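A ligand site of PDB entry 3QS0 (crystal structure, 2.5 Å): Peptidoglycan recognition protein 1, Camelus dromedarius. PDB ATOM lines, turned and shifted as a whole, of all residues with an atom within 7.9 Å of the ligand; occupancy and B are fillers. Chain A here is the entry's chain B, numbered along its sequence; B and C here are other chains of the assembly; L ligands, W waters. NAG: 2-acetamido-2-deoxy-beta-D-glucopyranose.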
ATOM      1  N   ASP A   2     -22.918  17.904 -25.346  1.00  0.00           N
ATOM      2  CA  ASP A   2     -21.888  17.343 -24.471  1.00  0.00           C
ATOM      3  C   ASP A   2     -22.319  15.894 -24.200  1.00  0.00           C
ATOM      4  O   ASP A   2     -23.295  15.429 -24.793  1.00  0.00           O
ATOM      5  CB  ASP A   2     -21.804  18.158 -23.159  1.00  0.00           C
ATOM      6  CG  ASP A   2     -23.031  18.009 -22.283  1.00  0.00           C
ATOM      7  OD1 ASP A   2     -23.063  17.060 -21.462  1.00  0.00           O
ATOM      8  OD2 ASP A   2     -23.971  18.833 -22.418  1.00  0.00           O
ATOM      9  N   PRO A   3     -21.594  15.162 -23.342  1.00  0.00           N
ATOM     10  CA  PRO A   3     -22.034  13.784 -23.088  1.00  0.00           C
ATOM     11  C   PRO A   3     -23.527  13.654 -22.788  1.00  0.00           C
ATOM     12  O   PRO A   3     -24.141  14.544 -22.190  1.00  0.00           O
ATOM     13  CB  PRO A   3     -21.143  13.366 -21.915  1.00  0.00           C
ATOM     14  CG  PRO A   3     -19.844  14.037 -22.267  1.00  0.00           C
ATOM     15  CD  PRO A   3     -20.310  15.435 -22.654  1.00  0.00           C
ATOM     16  N   PRO A   4     -24.139  12.541 -23.220  1.00  0.00           N
ATOM     17  CA  PRO A   4     -25.573  12.370 -22.957  1.00  0.00           C
ATOM     18  C   PRO A   4     -26.010  12.380 -21.495  1.00  0.00           C
ATOM     19  O   PRO A   4     -25.184  12.486 -20.568  1.00  0.00           O
ATOM     20  CB  PRO A   4     -25.886  11.014 -23.605  1.00  0.00           C
ATOM     21  CG  PRO A   4     -24.547  10.321 -23.677  1.00  0.00           C
ATOM     22  CD  PRO A   4     -23.637  11.449 -24.074  1.00  0.00           C
ATOM     23  N   ALA A   5     -27.323  12.261 -21.289  1.00  0.00           N
ATOM     24  CA  ALA A   5     -27.916  12.315 -19.965  1.00  0.00           C
ATOM     25  C   ALA A   5     -27.762  11.115 -19.056  1.00  0.00           C
ATOM     26  O   ALA A   5     -27.653   9.966 -19.499  1.00  0.00           O
ATOM     27  CB  ALA A   5     -29.401  12.681 -20.101  1.00  0.00           C
ATOM     28  N   CYS A   6     -27.754  11.419 -17.773  1.00  0.00           N
ATOM     29  CA  CYS A   6     -27.663  10.392 -16.767  1.00  0.00           C
ATOM     30  C   CYS A   6     -28.984   9.636 -16.921  1.00  0.00           C
ATOM     31  O   CYS A   6     -29.955  10.180 -17.451  1.00  0.00           O
ATOM     32  CB  CYS A   6     -27.499  11.032 -15.375  1.00  0.00           C
ATOM     33  SG  CYS A   6     -28.726  12.270 -14.855  1.00  0.00           S
ATOM     34  N   GLY A   7     -29.013   8.383 -16.489  1.00  0.00           N
ATOM     35  CA  GLY A   7     -30.242   7.629 -16.634  1.00  0.00           C
ATOM     36  C   GLY A   7     -30.381   6.991 -18.011  1.00  0.00           C
ATOM     37  O   GLY A   7     -31.320   6.229 -18.251  1.00  0.00           O
ATOM     38  N   SER A   8     -29.443   7.302 -18.911  1.00  0.00           N
ATOM     39  CA  SER A   8     -29.463   6.729 -20.263  1.00  0.00           C
ATOM     40  C   SER A   8     -30.870   6.704 -20.806  1.00  0.00           C
ATOM     41  O   SER A   8     -31.392   5.663 -21.178  1.00  0.00           O
ATOM     42  CB  SER A   8     -28.908   5.299 -20.235  1.00  0.00           C
ATOM     43  OG  SER A   8     -27.547   5.267 -19.877  1.00  0.00           O
ATOM     44  N   ARG A  28     -39.409  22.192 -10.422  1.00  0.00           N
ATOM     45  CA  ARG A  28     -38.304  21.386  -9.898  1.00  0.00           C
ATOM     46  C   ARG A  28     -37.343  22.270  -9.111  1.00  0.00           C
ATOM     47  O   ARG A  28     -37.069  23.395  -9.518  1.00  0.00           O
ATOM     48  CB  ARG A  28     -37.540  20.711 -11.038  1.00  0.00           C
ATOM     49  CG  ARG A  28     -37.036  21.707 -12.075  1.00  0.00           C
ATOM     50  CD  ARG A  28     -35.525  21.828 -12.107  1.00  0.00           C
ATOM     51  NE  ARG A  28     -34.929  21.032 -13.187  1.00  0.00           N
ATOM     52  CZ  ARG A  28     -33.657  21.133 -13.570  1.00  0.00           C
ATOM     53  NH1 ARG A  28     -32.839  21.981 -12.953  1.00  0.00           N
ATOM     54  NH2 ARG A  28     -33.196  20.380 -14.565  1.00  0.00           N
ATOM     55  N   ALA A 129     -32.449   8.844  -9.226  1.00  0.00           N
ATOM     56  CA  ALA A 129     -31.229   9.422  -8.673  1.00  0.00           C
ATOM     57  C   ALA A 129     -30.705  10.494  -9.635  1.00  0.00           C
ATOM     58  O   ALA A 129     -30.288  11.584  -9.216  1.00  0.00           O
ATOM     59  CB  ALA A 129     -30.188   8.336  -8.464  1.00  0.00           C
ATOM     60  N   CYS A 130     -30.745  10.164 -10.914  1.00  0.00           N
ATOM     61  CA  CYS A 130     -30.298  11.038 -11.996  1.00  0.00           C
ATOM     62  C   CYS A 130     -31.129  12.303 -11.972  1.00  0.00           C
ATOM     63  O   CYS A 130     -30.755  13.327 -12.538  1.00  0.00           O
ATOM     64  CB  CYS A 130     -30.468  10.275 -13.312  1.00  0.00           C
ATOM     65  SG  CYS A 130     -30.466  11.216 -14.854  1.00  0.00           S
ATOM     66  N   GLY A 131     -32.265  12.227 -11.297  1.00  0.00           N
ATOM     67  CA  GLY A 131     -33.146  13.372 -11.220  1.00  0.00           C
ATOM     68  C   GLY A 131     -32.570  14.409 -10.290  1.00  0.00           C
ATOM     69  O   GLY A 131     -32.392  15.569 -10.688  1.00  0.00           O
ATOM     70  N   VAL A 132     -32.278  13.997  -9.069  1.00  0.00           N
ATOM     71  CA  VAL A 132     -31.704  14.904  -8.082  1.00  0.00           C
ATOM     72  C   VAL A 132     -30.344  15.334  -8.596  1.00  0.00           C
ATOM     73  O   VAL A 132     -29.950  16.500  -8.448  1.00  0.00           O
ATOM     74  CB  VAL A 132     -31.535  14.220  -6.726  1.00  0.00           C
ATOM     75  CG1 VAL A 132     -31.039  15.221  -5.704  1.00  0.00           C
ATOM     76  CG2 VAL A 132     -32.859  13.620  -6.285  1.00  0.00           C
ATOM     77  N   ALA A 133     -29.626  14.400  -9.208  1.00  0.00           N
ATOM     78  CA  ALA A 133     -28.314  14.698  -9.750  1.00  0.00           C
ATOM     79  C   ALA A 133     -28.452  15.967 -10.560  1.00  0.00           C
ATOM     80  O   ALA A 133     -27.695  16.916 -10.395  1.00  0.00           O
ATOM     81  CB  ALA A 133     -27.822  13.569 -10.625  1.00  0.00           C
ATOM     82  N   LEU A 134     -29.447  15.984 -11.439  1.00  0.00           N
ATOM     83  CA  LEU A 134     -29.723  17.132 -12.292  1.00  0.00           C
ATOM     84  C   LEU A 134     -30.396  18.217 -11.485  1.00  0.00           C
ATOM     85  O   LEU A 134     -30.384  19.387 -11.879  1.00  0.00           O
ATOM     86  CB  LEU A 134     -30.639  16.723 -13.456  1.00  0.00           C
ATOM     87  CG  LEU A 134     -30.033  16.025 -14.667  1.00  0.00           C
ATOM     88  CD1 LEU A 134     -31.156  15.400 -15.486  1.00  0.00           C
ATOM     89  CD2 LEU A 134     -29.246  17.018 -15.520  1.00  0.00           C
ATOM     90  N   GLY A 135     -30.993  17.843 -10.366  1.00  0.00           N
ATOM     91  CA  GLY A 135     -31.660  18.818  -9.529  1.00  0.00           C
ATOM     92  C   GLY A 135     -33.092  19.046  -9.972  1.00  0.00           C
ATOM     93  O   GLY A 135     -33.611  20.168  -9.926  1.00  0.00           O
ATOM     94  N   PRO B  29     -26.076  25.299 -21.751  1.00  0.00           N
ATOM     95  CA  PRO B  29     -25.419  26.184 -20.782  1.00  0.00           C
ATOM     96  C   PRO B  29     -24.017  25.730 -20.351  1.00  0.00           C
ATOM     97  O   PRO B  29     -23.785  24.537 -20.133  1.00  0.00           O
ATOM     98  CB  PRO B  29     -26.411  26.175 -19.622  1.00  0.00           C
ATOM     99  CG  PRO B  29     -26.857  24.733 -19.628  1.00  0.00           C
ATOM    100  CD  PRO B  29     -27.165  24.523 -21.119  1.00  0.00           C
ATOM    101  N   ARG B  31     -20.992  25.341 -17.725  1.00  0.00           N
ATOM    102  CA  ARG B  31     -20.960  25.036 -16.307  1.00  0.00           C
ATOM    103  C   ARG B  31     -19.821  25.681 -15.557  1.00  0.00           C
ATOM    104  O   ARG B  31     -19.933  25.917 -14.353  1.00  0.00           O
ATOM    105  CB  ARG B  31     -20.850  23.522 -16.120  1.00  0.00           C
ATOM    106  CG  ARG B  31     -20.718  23.042 -14.682  1.00  0.00           C
ATOM    107  CD  ARG B  31     -20.589  21.523 -14.641  1.00  0.00           C
ATOM    108  NE  ARG B  31     -21.700  20.881 -15.353  1.00  0.00           N
ATOM    109  CZ  ARG B  31     -22.865  20.567 -14.794  1.00  0.00           C
ATOM    110  NH1 ARG B  31     -23.126  20.888 -13.535  1.00  0.00           N
ATOM    111  NH2 ARG B  31     -23.795  19.945 -15.506  1.00  0.00           N
ATOM    112  N   ARG B 138     -24.796  27.791 -16.563  1.00  0.00           N
ATOM    113  CA  ARG B 138     -25.745  27.025 -15.751  1.00  0.00           C
ATOM    114  C   ARG B 138     -26.095  27.815 -14.506  1.00  0.00           C
ATOM    115  O   ARG B 138     -25.318  28.661 -14.061  1.00  0.00           O
ATOM    116  CB  ARG B 138     -25.151  25.664 -15.349  1.00  0.00           C
ATOM    117  CG  ARG B 138     -25.189  24.630 -16.474  1.00  0.00           C
ATOM    118  CD  ARG B 138     -24.984  23.192 -15.968  1.00  0.00           C
ATOM    119  NE  ARG B 138     -24.980  22.234 -17.078  1.00  0.00           N
ATOM    120  CZ  ARG B 138     -26.059  21.834 -17.750  1.00  0.00           C
ATOM    121  NH1 ARG B 138     -27.273  22.159 -17.334  1.00  0.00           N
ATOM    122  NH2 ARG B 138     -25.908  21.133 -18.877  1.00  0.00           N
ATOM    123  N   ASN B 140     -26.189  26.761 -11.654  1.00  0.00           N
ATOM    124  CA  ASN B 140     -25.208  26.360 -10.651  1.00  0.00           C
ATOM    125  C   ASN B 140     -23.786  26.223 -11.230  1.00  0.00           C
ATOM    126  O   ASN B 140     -23.074  25.265 -10.934  1.00  0.00           O
ATOM    127  CB  ASN B 140     -25.644  25.049  -9.997  1.00  0.00           C
ATOM    128  CG  ASN B 140     -25.560  23.848 -10.937  1.00  0.00           C
ATOM    129  OD1 ASN B 140     -25.692  23.982 -12.154  1.00  0.00           O
ATOM    130  ND2 ASN B 140     -25.353  22.659 -10.357  1.00  0.00           N
ATOM    131  N   PRO C   4     -23.665   8.450  -4.437  1.00  0.00           N
ATOM    132  CA  PRO C   4     -24.365   8.195  -5.706  1.00  0.00           C
ATOM    133  C   PRO C   4     -24.033   6.857  -6.380  1.00  0.00           C
ATOM    134  O   PRO C   4     -23.407   6.854  -7.433  1.00  0.00           O
ATOM    135  CB  PRO C   4     -23.998   9.395  -6.575  1.00  0.00           C
ATOM    136  CG  PRO C   4     -22.698   9.852  -6.005  1.00  0.00           C
ATOM    137  CD  PRO C   4     -22.962   9.772  -4.515  1.00  0.00           C
ATOM    138  N   CYS C   6     -24.082   4.630  -8.849  1.00  0.00           N
ATOM    139  CA  CYS C   6     -24.494   5.157 -10.139  1.00  0.00           C
ATOM    140  C   CYS C   6     -24.887   4.279 -11.345  1.00  0.00           C
ATOM    141  O   CYS C   6     -24.416   3.152 -11.531  1.00  0.00           O
ATOM    142  CB  CYS C   6     -23.445   6.218 -10.513  1.00  0.00           C
ATOM    143  SG  CYS C   6     -23.709   7.261 -11.965  1.00  0.00           S
ATOM    144  N   ASN C 126     -22.403   7.082 -19.978  1.00  0.00           N
ATOM    145  CA  ASN C 126     -23.018   7.176 -18.651  1.00  0.00           C
ATOM    146  C   ASN C 126     -22.190   6.417 -17.641  1.00  0.00           C
ATOM    147  O   ASN C 126     -22.016   6.852 -16.499  1.00  0.00           O
ATOM    148  CB  ASN C 126     -24.429   6.597 -18.682  1.00  0.00           C
ATOM    149  CG  ASN C 126     -25.476   7.599 -18.275  1.00  0.00           C
ATOM    150  OD1 ASN C 126     -25.212   8.814 -18.218  1.00  0.00           O
ATOM    151  ND2 ASN C 126     -26.689   7.114 -17.992  1.00  0.00           N
ATOM    152  N   ALA C 129     -19.160   8.565 -16.628  1.00  0.00           N
ATOM    153  CA  ALA C 129     -19.526   9.658 -15.734  1.00  0.00           C
ATOM    154  C   ALA C 129     -19.755   9.051 -14.374  1.00  0.00           C
ATOM    155  O   ALA C 129     -19.357   9.600 -13.342  1.00  0.00           O
ATOM    156  CB  ALA C 129     -20.787  10.326 -16.222  1.00  0.00           C
ATOM    157  N   CYS C 130     -20.429   7.916 -14.378  1.00  0.00           N
ATOM    158  CA  CYS C 130     -20.708   7.185 -13.158  1.00  0.00           C
ATOM    159  C   CYS C 130     -19.389   6.850 -12.484  1.00  0.00           C
ATOM    160  O   CYS C 130     -19.259   6.962 -11.269  1.00  0.00           O
ATOM    161  CB  CYS C 130     -21.463   5.897 -13.484  1.00  0.00           C
ATOM    162  SG  CYS C 130     -23.292   5.985 -13.478  1.00  0.00           S
ATOM    163  N   VAL C 132     -16.644   8.458 -12.644  1.00  0.00           N
ATOM    164  CA  VAL C 132     -16.093   9.657 -12.039  1.00  0.00           C
ATOM    165  C   VAL C 132     -16.779   9.925 -10.703  1.00  0.00           C
ATOM    166  O   VAL C 132     -16.111  10.086  -9.679  1.00  0.00           O
ATOM    167  CB  VAL C 132     -16.233  10.870 -12.971  1.00  0.00           C
ATOM    168  CG1 VAL C 132     -15.610  12.098 -12.328  1.00  0.00           C
ATOM    169  CG2 VAL C 132     -15.561  10.572 -14.310  1.00  0.00           C
ATOM    170  N   ALA C 133     -18.103   9.935 -10.719  1.00  0.00           N
ATOM    171  CA  ALA C 133     -18.884  10.163  -9.510  1.00  0.00           C
ATOM    172  C   ALA C 133     -18.430   9.236  -8.371  1.00  0.00           C
ATOM    173  O   ALA C 133     -18.286   9.662  -7.222  1.00  0.00           O
ATOM    174  CB  ALA C 133     -20.360   9.937  -9.801  1.00  0.00           C
HETATM  175  C1  NAG L   1     -25.546  16.739 -14.401  1.00  0.00           C
HETATM  176  C2  NAG L   1     -25.544  15.227 -14.662  1.00  0.00           C
HETATM  177  C3  NAG L   1     -25.271  14.767 -16.108  1.00  0.00           C
HETATM  178  C4  NAG L   1     -25.613  15.815 -17.189  1.00  0.00           C
HETATM  179  C5  NAG L   1     -25.250  17.205 -16.694  1.00  0.00           C
HETATM  180  C6  NAG L   1     -25.580  18.262 -17.699  1.00  0.00           C
HETATM  181  C7  NAG L   1     -24.321  13.369 -13.692  1.00  0.00           C
HETATM  182  C8  NAG L   1     -23.275  12.923 -12.692  1.00  0.00           C
HETATM  183  N2  NAG L   1     -24.520  14.673 -13.791  1.00  0.00           N
HETATM  184  O1  NAG L   1     -26.376  17.025 -13.321  1.00  0.00           O
HETATM  185  O3  NAG L   1     -26.016  13.595 -16.375  1.00  0.00           O
HETATM  186  O4  NAG L   1     -24.906  15.535 -18.396  1.00  0.00           O
HETATM  187  O5  NAG L   1     -26.020  17.476 -15.530  1.00  0.00           O
HETATM  188  O6  NAG L   1     -26.983  18.397 -17.832  1.00  0.00           O
HETATM  189  O7  NAG L   1     -24.929  12.547 -14.369  1.00  0.00           O
HETATM  190  O   HOH W   1     -24.581  10.951 -16.965  1.00  0.00           O
HETATM  191  O   HOH W   2     -28.687  16.487 -19.232  1.00  0.00           O
HETATM  192  O   HOH W   3     -21.941  15.776 -18.680  1.00  0.00           O
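Water W3 bridges an oxygen (O4) of the ligand (3.0 Å) and the side-chain carboxylate of Asp 2 (3.3 Å).
Water W1 lies within hydrogen-bond range of OD1 of Asn 126 of chain C (2.6 Å), O3 of the ligand (3.1 Å) and N of Cys 6 of chain A (3.3 Å).
Asp 2 touches the ligand.
O of Pro 3 touches O4 of the ligand, at 3.995 Å.
Pro 4 of chain A touches the ligand.
CD2 of Leu 134 touches O5 of the ligand, 3.3 Å away.
The nearest printed residue that does not touch the ligand is Ala 5 (4.05 Å).
N of Cys 6 of chain A lies within hydrogen-bond range of O3 of the ligand (3.1 Å).
The side-chain sulfur of Cys 6 of chain A sits close to an oxygen (O3) of the ligand, at 3.4 Å.
NH2 of Arg 138 of chain B lies within hydrogen-bond range of O6 of the ligand (3.1 Å).
An oxygen (O1) of the ligand lies within hydrogen-bond range of the backbone carbonyl oxygen (O) of Ala 133 of chain A (3.2 Å).
NH2 of Arg 31 of chain B lies close to O5 of the ligand.
The side-chain sulfur of Cys 6 of chain A forms a disulfide with the side-chain sulfur of Cys 130 of chain A.
The side-chain sulfur (SG) of Cys 130 of chain C is disulfide-bonded to the side-chain sulfur (SG) of Cys 6 of chain C.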
